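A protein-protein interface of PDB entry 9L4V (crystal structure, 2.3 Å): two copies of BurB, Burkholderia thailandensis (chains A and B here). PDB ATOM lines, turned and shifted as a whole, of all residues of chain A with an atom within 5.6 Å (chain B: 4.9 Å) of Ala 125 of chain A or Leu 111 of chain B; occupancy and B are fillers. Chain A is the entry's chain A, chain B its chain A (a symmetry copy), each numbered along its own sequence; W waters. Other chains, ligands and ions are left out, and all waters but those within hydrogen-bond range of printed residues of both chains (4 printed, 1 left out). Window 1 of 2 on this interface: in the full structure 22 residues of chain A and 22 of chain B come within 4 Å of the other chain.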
ATOM      1  N   HIS A  93     -37.328 -20.682 -18.419  1.00  0.00           N
ATOM      2  CA  HIS A  93     -36.549 -20.536 -17.202  1.00  0.00           C
ATOM      3  C   HIS A  93     -37.471 -20.447 -15.998  1.00  0.00           C
ATOM      4  O   HIS A  93     -38.561 -19.867 -16.064  1.00  0.00           O
ATOM      5  CB  HIS A  93     -35.678 -19.274 -17.237  1.00  0.00           C
ATOM      6  CG  HIS A  93     -35.119 -18.911 -15.896  1.00  0.00           C
ATOM      7  ND1 HIS A  93     -34.019 -19.547 -15.355  1.00  0.00           N
ATOM      8  CD2 HIS A  93     -35.542 -18.033 -14.956  1.00  0.00           C
ATOM      9  CE1 HIS A  93     -33.772 -19.055 -14.155  1.00  0.00           C
ATOM     10  NE2 HIS A  93     -34.682 -18.133 -13.891  1.00  0.00           N
ATOM     11  N   ASP A 123     -33.353 -24.009 -14.429  1.00  0.00           N
ATOM     12  CA  ASP A 123     -32.555 -22.821 -14.109  1.00  0.00           C
ATOM     13  C   ASP A 123     -31.542 -22.622 -15.236  1.00  0.00           C
ATOM     14  O   ASP A 123     -30.581 -23.391 -15.362  1.00  0.00           O
ATOM     15  CB  ASP A 123     -31.858 -22.982 -12.757  1.00  0.00           C
ATOM     16  CG  ASP A 123     -31.101 -21.724 -12.323  1.00  0.00           C
ATOM     17  OD1 ASP A 123     -31.069 -20.736 -13.091  1.00  0.00           O
ATOM     18  OD2 ASP A 123     -30.528 -21.724 -11.207  1.00  0.00           O
ATOM     19  N   TYR A 124     -31.754 -21.607 -16.069  1.00  0.00           N
ATOM     20  CA  TYR A 124     -30.796 -21.356 -17.149  1.00  0.00           C
ATOM     21  C   TYR A 124     -29.377 -21.206 -16.616  1.00  0.00           C
ATOM     22  O   TYR A 124     -28.413 -21.569 -17.302  1.00  0.00           O
ATOM     23  CB  TYR A 124     -31.165 -20.093 -17.932  1.00  0.00           C
ATOM     24  CG  TYR A 124     -32.347 -20.218 -18.884  1.00  0.00           C
ATOM     25  CD1 TYR A 124     -33.116 -21.376 -18.946  1.00  0.00           C
ATOM     26  CD2 TYR A 124     -32.706 -19.148 -19.695  1.00  0.00           C
ATOM     27  CE1 TYR A 124     -34.205 -21.464 -19.802  1.00  0.00           C
ATOM     28  CE2 TYR A 124     -33.785 -19.225 -20.558  1.00  0.00           C
ATOM     29  CZ  TYR A 124     -34.534 -20.380 -20.611  1.00  0.00           C
ATOM     30  OH  TYR A 124     -35.596 -20.446 -21.494  1.00  0.00           O
ATOM     31  N   ALA A 125     -29.219 -20.669 -15.407  1.00  0.00           N
ATOM     32  CA  ALA A 125     -27.865 -20.482 -14.901  1.00  0.00           C
ATOM     33  C   ALA A 125     -27.192 -21.796 -14.504  1.00  0.00           C
ATOM     34  O   ALA A 125     -25.975 -21.799 -14.274  1.00  0.00           O
ATOM     35  CB  ALA A 125     -27.863 -19.511 -13.719  1.00  0.00           C
ATOM     36  N   SER A 126     -27.944 -22.907 -14.451  1.00  0.00           N
ATOM     37  CA  SER A 126     -27.368 -24.185 -14.051  1.00  0.00           C
ATOM     38  C   SER A 126     -26.541 -24.821 -15.163  1.00  0.00           C
ATOM     39  O   SER A 126     -25.657 -25.624 -14.857  1.00  0.00           O
ATOM     40  CB  SER A 126     -28.468 -25.162 -13.600  1.00  0.00           C
ATOM     41  OG  SER A 126     -29.252 -25.598 -14.706  1.00  0.00           O
ATOM     42  N   THR A 127     -26.796 -24.479 -16.441  1.00  0.00           N
ATOM     43  CA  THR A 127     -26.004 -24.974 -17.567  1.00  0.00           C
ATOM     44  C   THR A 127     -25.254 -23.882 -18.343  1.00  0.00           C
ATOM     45  O   THR A 127     -24.280 -24.199 -19.039  1.00  0.00           O
ATOM     46  CB  THR A 127     -26.893 -25.741 -18.570  1.00  0.00           C
ATOM     47  OG1 THR A 127     -27.900 -24.867 -19.083  1.00  0.00           O
ATOM     48  CG2 THR A 127     -27.588 -26.970 -17.926  1.00  0.00           C
ATOM     49  N   GLU A 128     -25.662 -22.620 -18.246  1.00  0.00           N
ATOM     50  CA  GLU A 128     -25.177 -21.568 -19.137  1.00  0.00           C
ATOM     51  C   GLU A 128     -24.235 -20.617 -18.406  1.00  0.00           C
ATOM     52  O   GLU A 128     -24.588 -20.082 -17.353  1.00  0.00           O
ATOM     53  CB  GLU A 128     -26.357 -20.786 -19.721  1.00  0.00           C
ATOM     54  CG  GLU A 128     -27.460 -21.679 -20.298  1.00  0.00           C
ATOM     55  CD  GLU A 128     -26.953 -22.541 -21.441  1.00  0.00           C
ATOM     56  OE1 GLU A 128     -26.490 -21.962 -22.452  1.00  0.00           O
ATOM     57  OE2 GLU A 128     -26.993 -23.790 -21.320  1.00  0.00           O
ATOM     58  N   ARG A 145     -34.946 -14.225  -9.023  1.00  0.00           N
ATOM     59  CA  ARG A 145     -33.853 -13.290  -9.218  1.00  0.00           C
ATOM     60  C   ARG A 145     -34.331 -12.029  -9.925  1.00  0.00           C
ATOM     61  O   ARG A 145     -33.584 -11.050  -9.967  1.00  0.00           O
ATOM     62  CB  ARG A 145     -32.731 -13.967 -10.016  1.00  0.00           C
ATOM     63  CG  ARG A 145     -32.262 -15.275  -9.406  1.00  0.00           C
ATOM     64  CD  ARG A 145     -31.083 -15.862 -10.188  1.00  0.00           C
ATOM     65  NE  ARG A 145     -30.821 -17.220  -9.739  1.00  0.00           N
ATOM     66  CZ  ARG A 145     -30.820 -18.286 -10.527  1.00  0.00           C
ATOM     67  NH1 ARG A 145     -30.868 -18.175 -11.848  1.00  0.00           N
ATOM     68  NH2 ARG A 145     -30.751 -19.494  -9.975  1.00  0.00           N
ATOM     69  N   THR A 149     -29.701 -14.042 -15.949  1.00  0.00           N
ATOM     70  CA  THR A 149     -28.430 -14.064 -16.668  1.00  0.00           C
ATOM     71  C   THR A 149     -27.871 -15.479 -16.640  1.00  0.00           C
ATOM     72  O   THR A 149     -28.376 -16.359 -15.937  1.00  0.00           O
ATOM     73  CB  THR A 149     -27.400 -13.137 -16.017  1.00  0.00           C
ATOM     74  OG1 THR A 149     -27.236 -13.547 -14.651  1.00  0.00           O
ATOM     75  CG2 THR A 149     -27.859 -11.678 -16.041  1.00  0.00           C
ATOM     76  N   GLY A 150     -26.796 -15.694 -17.394  1.00  0.00           N
ATOM     77  CA  GLY A 150     -25.974 -16.858 -17.159  1.00  0.00           C
ATOM     78  C   GLY A 150     -25.361 -16.825 -15.773  1.00  0.00           C
ATOM     79  O   GLY A 150     -25.345 -15.801 -15.086  1.00  0.00           O
ATOM     80  N   ALA A 151     -24.836 -17.971 -15.349  1.00  0.00           N
ATOM     81  CA  ALA A 151     -24.226 -18.004 -14.028  1.00  0.00           C
ATOM     82  C   ALA A 151     -22.986 -17.117 -13.963  1.00  0.00           C
ATOM     83  O   ALA A 151     -22.690 -16.552 -12.907  1.00  0.00           O
ATOM     84  CB  ALA A 151     -23.876 -19.441 -13.638  1.00  0.00           C
ATOM     85  N   ARG B  54     -24.039 -10.743  -7.147  1.00  0.00           N
ATOM     86  CA  ARG B  54     -24.382 -11.844  -8.032  1.00  0.00           C
ATOM     87  C   ARG B  54     -23.544 -11.796  -9.300  1.00  0.00           C
ATOM     88  O   ARG B  54     -23.152 -10.731  -9.777  1.00  0.00           O
ATOM     89  CB  ARG B  54     -25.874 -11.816  -8.386  1.00  0.00           C
ATOM     90  CG  ARG B  54     -26.318 -10.616  -9.196  1.00  0.00           C
ATOM     91  CD  ARG B  54     -27.773 -10.766  -9.654  1.00  0.00           C
ATOM     92  NE  ARG B  54     -27.862 -11.608 -10.840  1.00  0.00           N
ATOM     93  CZ  ARG B  54     -28.981 -11.884 -11.497  1.00  0.00           C
ATOM     94  NH1 ARG B  54     -30.157 -11.419 -11.096  1.00  0.00           N
ATOM     95  NH2 ARG B  54     -28.914 -12.621 -12.602  1.00  0.00           N
ATOM     96  N   PRO B  97     -30.743 -22.276  -4.283  1.00  0.00           N
ATOM     97  CA  PRO B  97     -29.341 -21.988  -4.016  1.00  0.00           C
ATOM     98  C   PRO B  97     -28.797 -20.584  -4.289  1.00  0.00           C
ATOM     99  O   PRO B  97     -29.242 -19.929  -5.195  1.00  0.00           O
ATOM    100  CB  PRO B  97     -28.647 -22.999  -4.900  1.00  0.00           C
ATOM    101  CG  PRO B  97     -29.558 -23.215  -6.041  1.00  0.00           C
ATOM    102  CD  PRO B  97     -30.926 -23.142  -5.458  1.00  0.00           C
ATOM    103  N   ASN B  98     -27.836 -20.124  -3.501  1.00  0.00           N
ATOM    104  CA  ASN B  98     -27.220 -18.837  -3.801  1.00  0.00           C
ATOM    105  C   ASN B  98     -25.894 -18.929  -4.550  1.00  0.00           C
ATOM    106  O   ASN B  98     -25.377 -17.884  -4.973  1.00  0.00           O
ATOM    107  CB  ASN B  98     -27.026 -18.007  -2.515  1.00  0.00           C
ATOM    108  CG  ASN B  98     -26.159 -18.694  -1.471  1.00  0.00           C
ATOM    109  OD1 ASN B  98     -25.435 -19.650  -1.750  1.00  0.00           O
ATOM    110  ND2 ASN B  98     -26.249 -18.203  -0.234  1.00  0.00           N
ATOM    111  N   VAL B  99     -25.328 -20.129  -4.732  1.00  0.00           N
ATOM    112  CA  VAL B  99     -24.111 -20.307  -5.526  1.00  0.00           C
ATOM    113  C   VAL B  99     -24.288 -21.464  -6.501  1.00  0.00           C
ATOM    114  O   VAL B  99     -25.070 -22.392  -6.264  1.00  0.00           O
ATOM    115  CB  VAL B  99     -22.869 -20.570  -4.650  1.00  0.00           C
ATOM    116  CG1 VAL B  99     -22.655 -19.438  -3.672  1.00  0.00           C
ATOM    117  CG2 VAL B  99     -22.976 -21.947  -3.938  1.00  0.00           C
ATOM    118  N   ARG B 100     -23.543 -21.417  -7.603  1.00  0.00           N
ATOM    119  CA  ARG B 100     -23.416 -22.563  -8.501  1.00  0.00           C
ATOM    120  C   ARG B 100     -21.984 -23.065  -8.444  1.00  0.00           C
ATOM    121  O   ARG B 100     -21.044 -22.274  -8.563  1.00  0.00           O
ATOM    122  CB  ARG B 100     -23.762 -22.221  -9.954  1.00  0.00           C
ATOM    123  CG  ARG B 100     -23.209 -23.303 -10.939  1.00  0.00           C
ATOM    124  CD  ARG B 100     -23.919 -23.360 -12.271  1.00  0.00           C
ATOM    125  NE  ARG B 100     -23.196 -24.217 -13.212  1.00  0.00           N
ATOM    126  CZ  ARG B 100     -23.105 -23.978 -14.514  1.00  0.00           C
ATOM    127  NH1 ARG B 100     -23.729 -22.956 -15.066  1.00  0.00           N
ATOM    128  NH2 ARG B 100     -22.336 -24.760 -15.273  1.00  0.00           N
ATOM    129  N   TRP B 109     -19.580 -19.786  -8.313  1.00  0.00           N
ATOM    130  CA  TRP B 109     -20.113 -18.481  -8.723  1.00  0.00           C
ATOM    131  C   TRP B 109     -21.383 -18.119  -7.955  1.00  0.00           C
ATOM    132  O   TRP B 109     -22.246 -18.968  -7.707  1.00  0.00           O
ATOM    133  CB  TRP B 109     -20.431 -18.425 -10.231  1.00  0.00           C
ATOM    134  CG  TRP B 109     -19.218 -18.403 -11.133  1.00  0.00           C
ATOM    135  CD1 TRP B 109     -18.388 -19.459 -11.413  1.00  0.00           C
ATOM    136  CD2 TRP B 109     -18.717 -17.286 -11.887  1.00  0.00           C
ATOM    137  NE1 TRP B 109     -17.404 -19.064 -12.298  1.00  0.00           N
ATOM    138  CE2 TRP B 109     -17.579 -17.738 -12.601  1.00  0.00           C
ATOM    139  CE3 TRP B 109     -19.123 -15.953 -12.038  1.00  0.00           C
ATOM    140  CZ2 TRP B 109     -16.832 -16.893 -13.442  1.00  0.00           C
ATOM    141  CZ3 TRP B 109     -18.375 -15.106 -12.885  1.00  0.00           C
ATOM    142  CH2 TRP B 109     -17.248 -15.585 -13.571  1.00  0.00           C
ATOM    143  N   SER B 110     -21.514 -16.836  -7.616  1.00  0.00           N
ATOM    144  CA  SER B 110     -22.702 -16.361  -6.910  1.00  0.00           C
ATOM    145  C   SER B 110     -23.900 -16.328  -7.862  1.00  0.00           C
ATOM    146  O   SER B 110     -23.841 -15.694  -8.919  1.00  0.00           O
ATOM    147  CB  SER B 110     -22.434 -14.972  -6.335  1.00  0.00           C
ATOM    148  OG  SER B 110     -21.895 -14.109  -7.339  1.00  0.00           O
ATOM    149  N   LEU B 111     -24.979 -17.033  -7.510  1.00  0.00           N
ATOM    150  CA  LEU B 111     -26.213 -16.908  -8.272  1.00  0.00           C
ATOM    151  C   LEU B 111     -27.040 -15.710  -7.829  1.00  0.00           C
ATOM    152  O   LEU B 111     -27.919 -15.272  -8.573  1.00  0.00           O
ATOM    153  CB  LEU B 111     -27.054 -18.180  -8.155  1.00  0.00           C
ATOM    154  CG  LEU B 111     -26.404 -19.405  -8.804  1.00  0.00           C
ATOM    155  CD1 LEU B 111     -27.077 -20.715  -8.333  1.00  0.00           C
ATOM    156  CD2 LEU B 111     -26.391 -19.269 -10.341  1.00  0.00           C
ATOM    157  N   ARG B 112     -26.782 -15.167  -6.645  1.00  0.00           N
ATOM    158  CA  ARG B 112     -27.441 -13.941  -6.219  1.00  0.00           C
ATOM    159  C   ARG B 112     -26.478 -13.148  -5.351  1.00  0.00           C
ATOM    160  O   ARG B 112     -25.358 -13.595  -5.050  1.00  0.00           O
ATOM    161  CB  ARG B 112     -28.759 -14.211  -5.481  1.00  0.00           C
ATOM    162  CG  ARG B 112     -28.741 -15.354  -4.532  1.00  0.00           C
ATOM    163  CD  ARG B 112     -30.185 -15.746  -4.166  1.00  0.00           C
ATOM    164  NE  ARG B 112     -30.759 -16.700  -5.115  1.00  0.00           N
ATOM    165  CZ  ARG B 112     -32.045 -16.765  -5.450  1.00  0.00           C
ATOM    166  NH1 ARG B 112     -32.934 -15.905  -4.972  1.00  0.00           N
ATOM    167  NH2 ARG B 112     -32.451 -17.722  -6.284  1.00  0.00           N
ATOM    168  N   ASP B 113     -26.914 -11.933  -4.997  1.00  0.00           N
ATOM    169  CA  ASP B 113     -26.204 -11.150  -4.000  1.00  0.00           C
ATOM    170  C   ASP B 113     -26.181 -11.939  -2.708  1.00  0.00           C
ATOM    171  O   ASP B 113     -27.219 -12.422  -2.242  1.00  0.00           O
ATOM    172  CB  ASP B 113     -26.877  -9.790  -3.775  1.00  0.00           C
ATOM    173  CG  ASP B 113     -26.951  -8.973  -5.030  1.00  0.00           C
ATOM    174  OD1 ASP B 113     -26.186  -9.262  -5.963  1.00  0.00           O
ATOM    175  OD2 ASP B 113     -27.786  -8.046  -5.100  1.00  0.00           O
HETATM  176  O   HOH W   1     -31.244 -20.015  -6.733  1.00  0.00           O
HETATM  177  O   HOH W   2     -24.852 -15.498 -11.413  1.00  0.00           O
HETATM  178  O   HOH W   3     -25.587 -12.690 -12.026  1.00  0.00           O
HETATM  179  O   HOH W   4     -25.539 -26.361 -11.976  1.00  0.00           O
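The backbone carbonyl oxygen (O) of Ser 126 of chain A lies close to the guanidinium group (NE) of Arg 100 of chain B, 3.3 Å away. OG1 of Thr 149 of chain A sits at hydrogen-bond distance from NH2 of Arg 54 of chain B (2.8 Å). O of Ala 125 of chain A sits at hydrogen-bond distance from NH1 of Arg 100 of chain B, at 2.6 Å.
No position is printed for both chains. Of the 11 pairs that touch across the chains among the printed residues, none has its exchanged pair printed and touching as well.
Of chain B, only Arg 100 (2.6 Å) and Leu 111 (3.7 Å) come within 4 Å of Ala 125 of chain A. Of the printed residues of chain B, Ser 126 of chain A touches Arg 100 (3.1 Å). Of the printed residues of chain B, Thr 127 of chain A touches Arg 100. Of the printed residues of chain B, Glu 128 of chain A touches Arg 100 (3.7 Å). Pro 97 of chain B touches none of the printed residues of chain A. Asn 98 of chain B touches none of the printed residues of chain A. Of chain A, only Ala 125 and Arg 145 come within 4 Å of Leu 111 of chain B. Printed residues of chain A within 4 Å of Arg 112 of chain B: Arg 145 (3.9 Å). The nearest printed residue of chain B that does not touch Ala 125 of chain A is Arg 54 of chain B (7.1 Å). The nearest residue of chain A that does not touch Leu 111 of chain B is Ala 151 of chain A (4.2 Å). The nearest printed residue of chain B that does not touch Arg 145 of chain A is Pro 97 of chain B (5.0 Å).
Of the 10 printed residues of chain B, 5 touch a printed residue of chain A. Hydrophobic or aromatic side chains of chain A within 4 Å of the printed part of chain B: Ala 125 and Ala 151.
Water W1 lies within hydrogen-bond range of O of Pro 97 of chain B (2.5 Å), NH2 of Arg 112 of chain B (2.6 Å) and NH2 of Arg 145 of chain A (3.3 Å). Water W2 lies within hydrogen-bond range of O of Ser 110 of chain B (2.7 Å) and O of Ala 151 of chain A (2.8 Å). Water W3 bridges NE of Arg 54 of chain B (2.8 Å) and OG1 of Thr 149 of chain A (3.2 Å). Water W4 bridges the backbone carbonyl oxygen (O) of Ser 126 of chain A (3.0 Å) and the guanidinium group (NE) of Arg 100 of chain B (3.4 Å).
Among the printed residues, pairs that only touch across the chains: Ala 125 of chain A with Leu 111 of chain B, Thr 127 of chain A with Arg 100 of chain B, Glu 128 of chain A with Arg 100 of chain B, Arg 145 of chain A with Arg 54 of chain B, Arg 145 of chain A with Leu 111 of chain B, Arg 145 of chain A with Arg 112 of chain B, Ala 151 of chain A with Arg 100 of chain B and Ala 151 of chain A with Trp 109 of chain B.
The backbone carbonyl oxygen (O) of Asn 98 of chain B lies within hydrogen-bond range of the backbone NH (N) of Arg 112 of chain B (3.5 Å). The backbone NH (N) of Arg 54 of chain B is in hydrogen-bond range of the side-chain carboxylate (OD1) of Asp 113 of chain B (2.9 Å). The backbone NH (N) of Ala 125 of chain A sits at hydrogen-bond distance from the side-chain carboxylate (OD1) of Asp 123 of chain A (3.0 Å). The backbone carbonyl oxygen (O) of Asn 98 of chain B sits at hydrogen-bond distance from the backbone NH (N) of Leu 111 of chain B. N of Ala 151 of chain A is in hydrogen-bond range of O of Glu 128 of chain A. The side-chain carboxylate (OE2) of Glu 128 of chain A sits at hydrogen-bond distance from the side-chain hydroxyl (OG1) of Thr 127 of chain A (2.6 Å).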
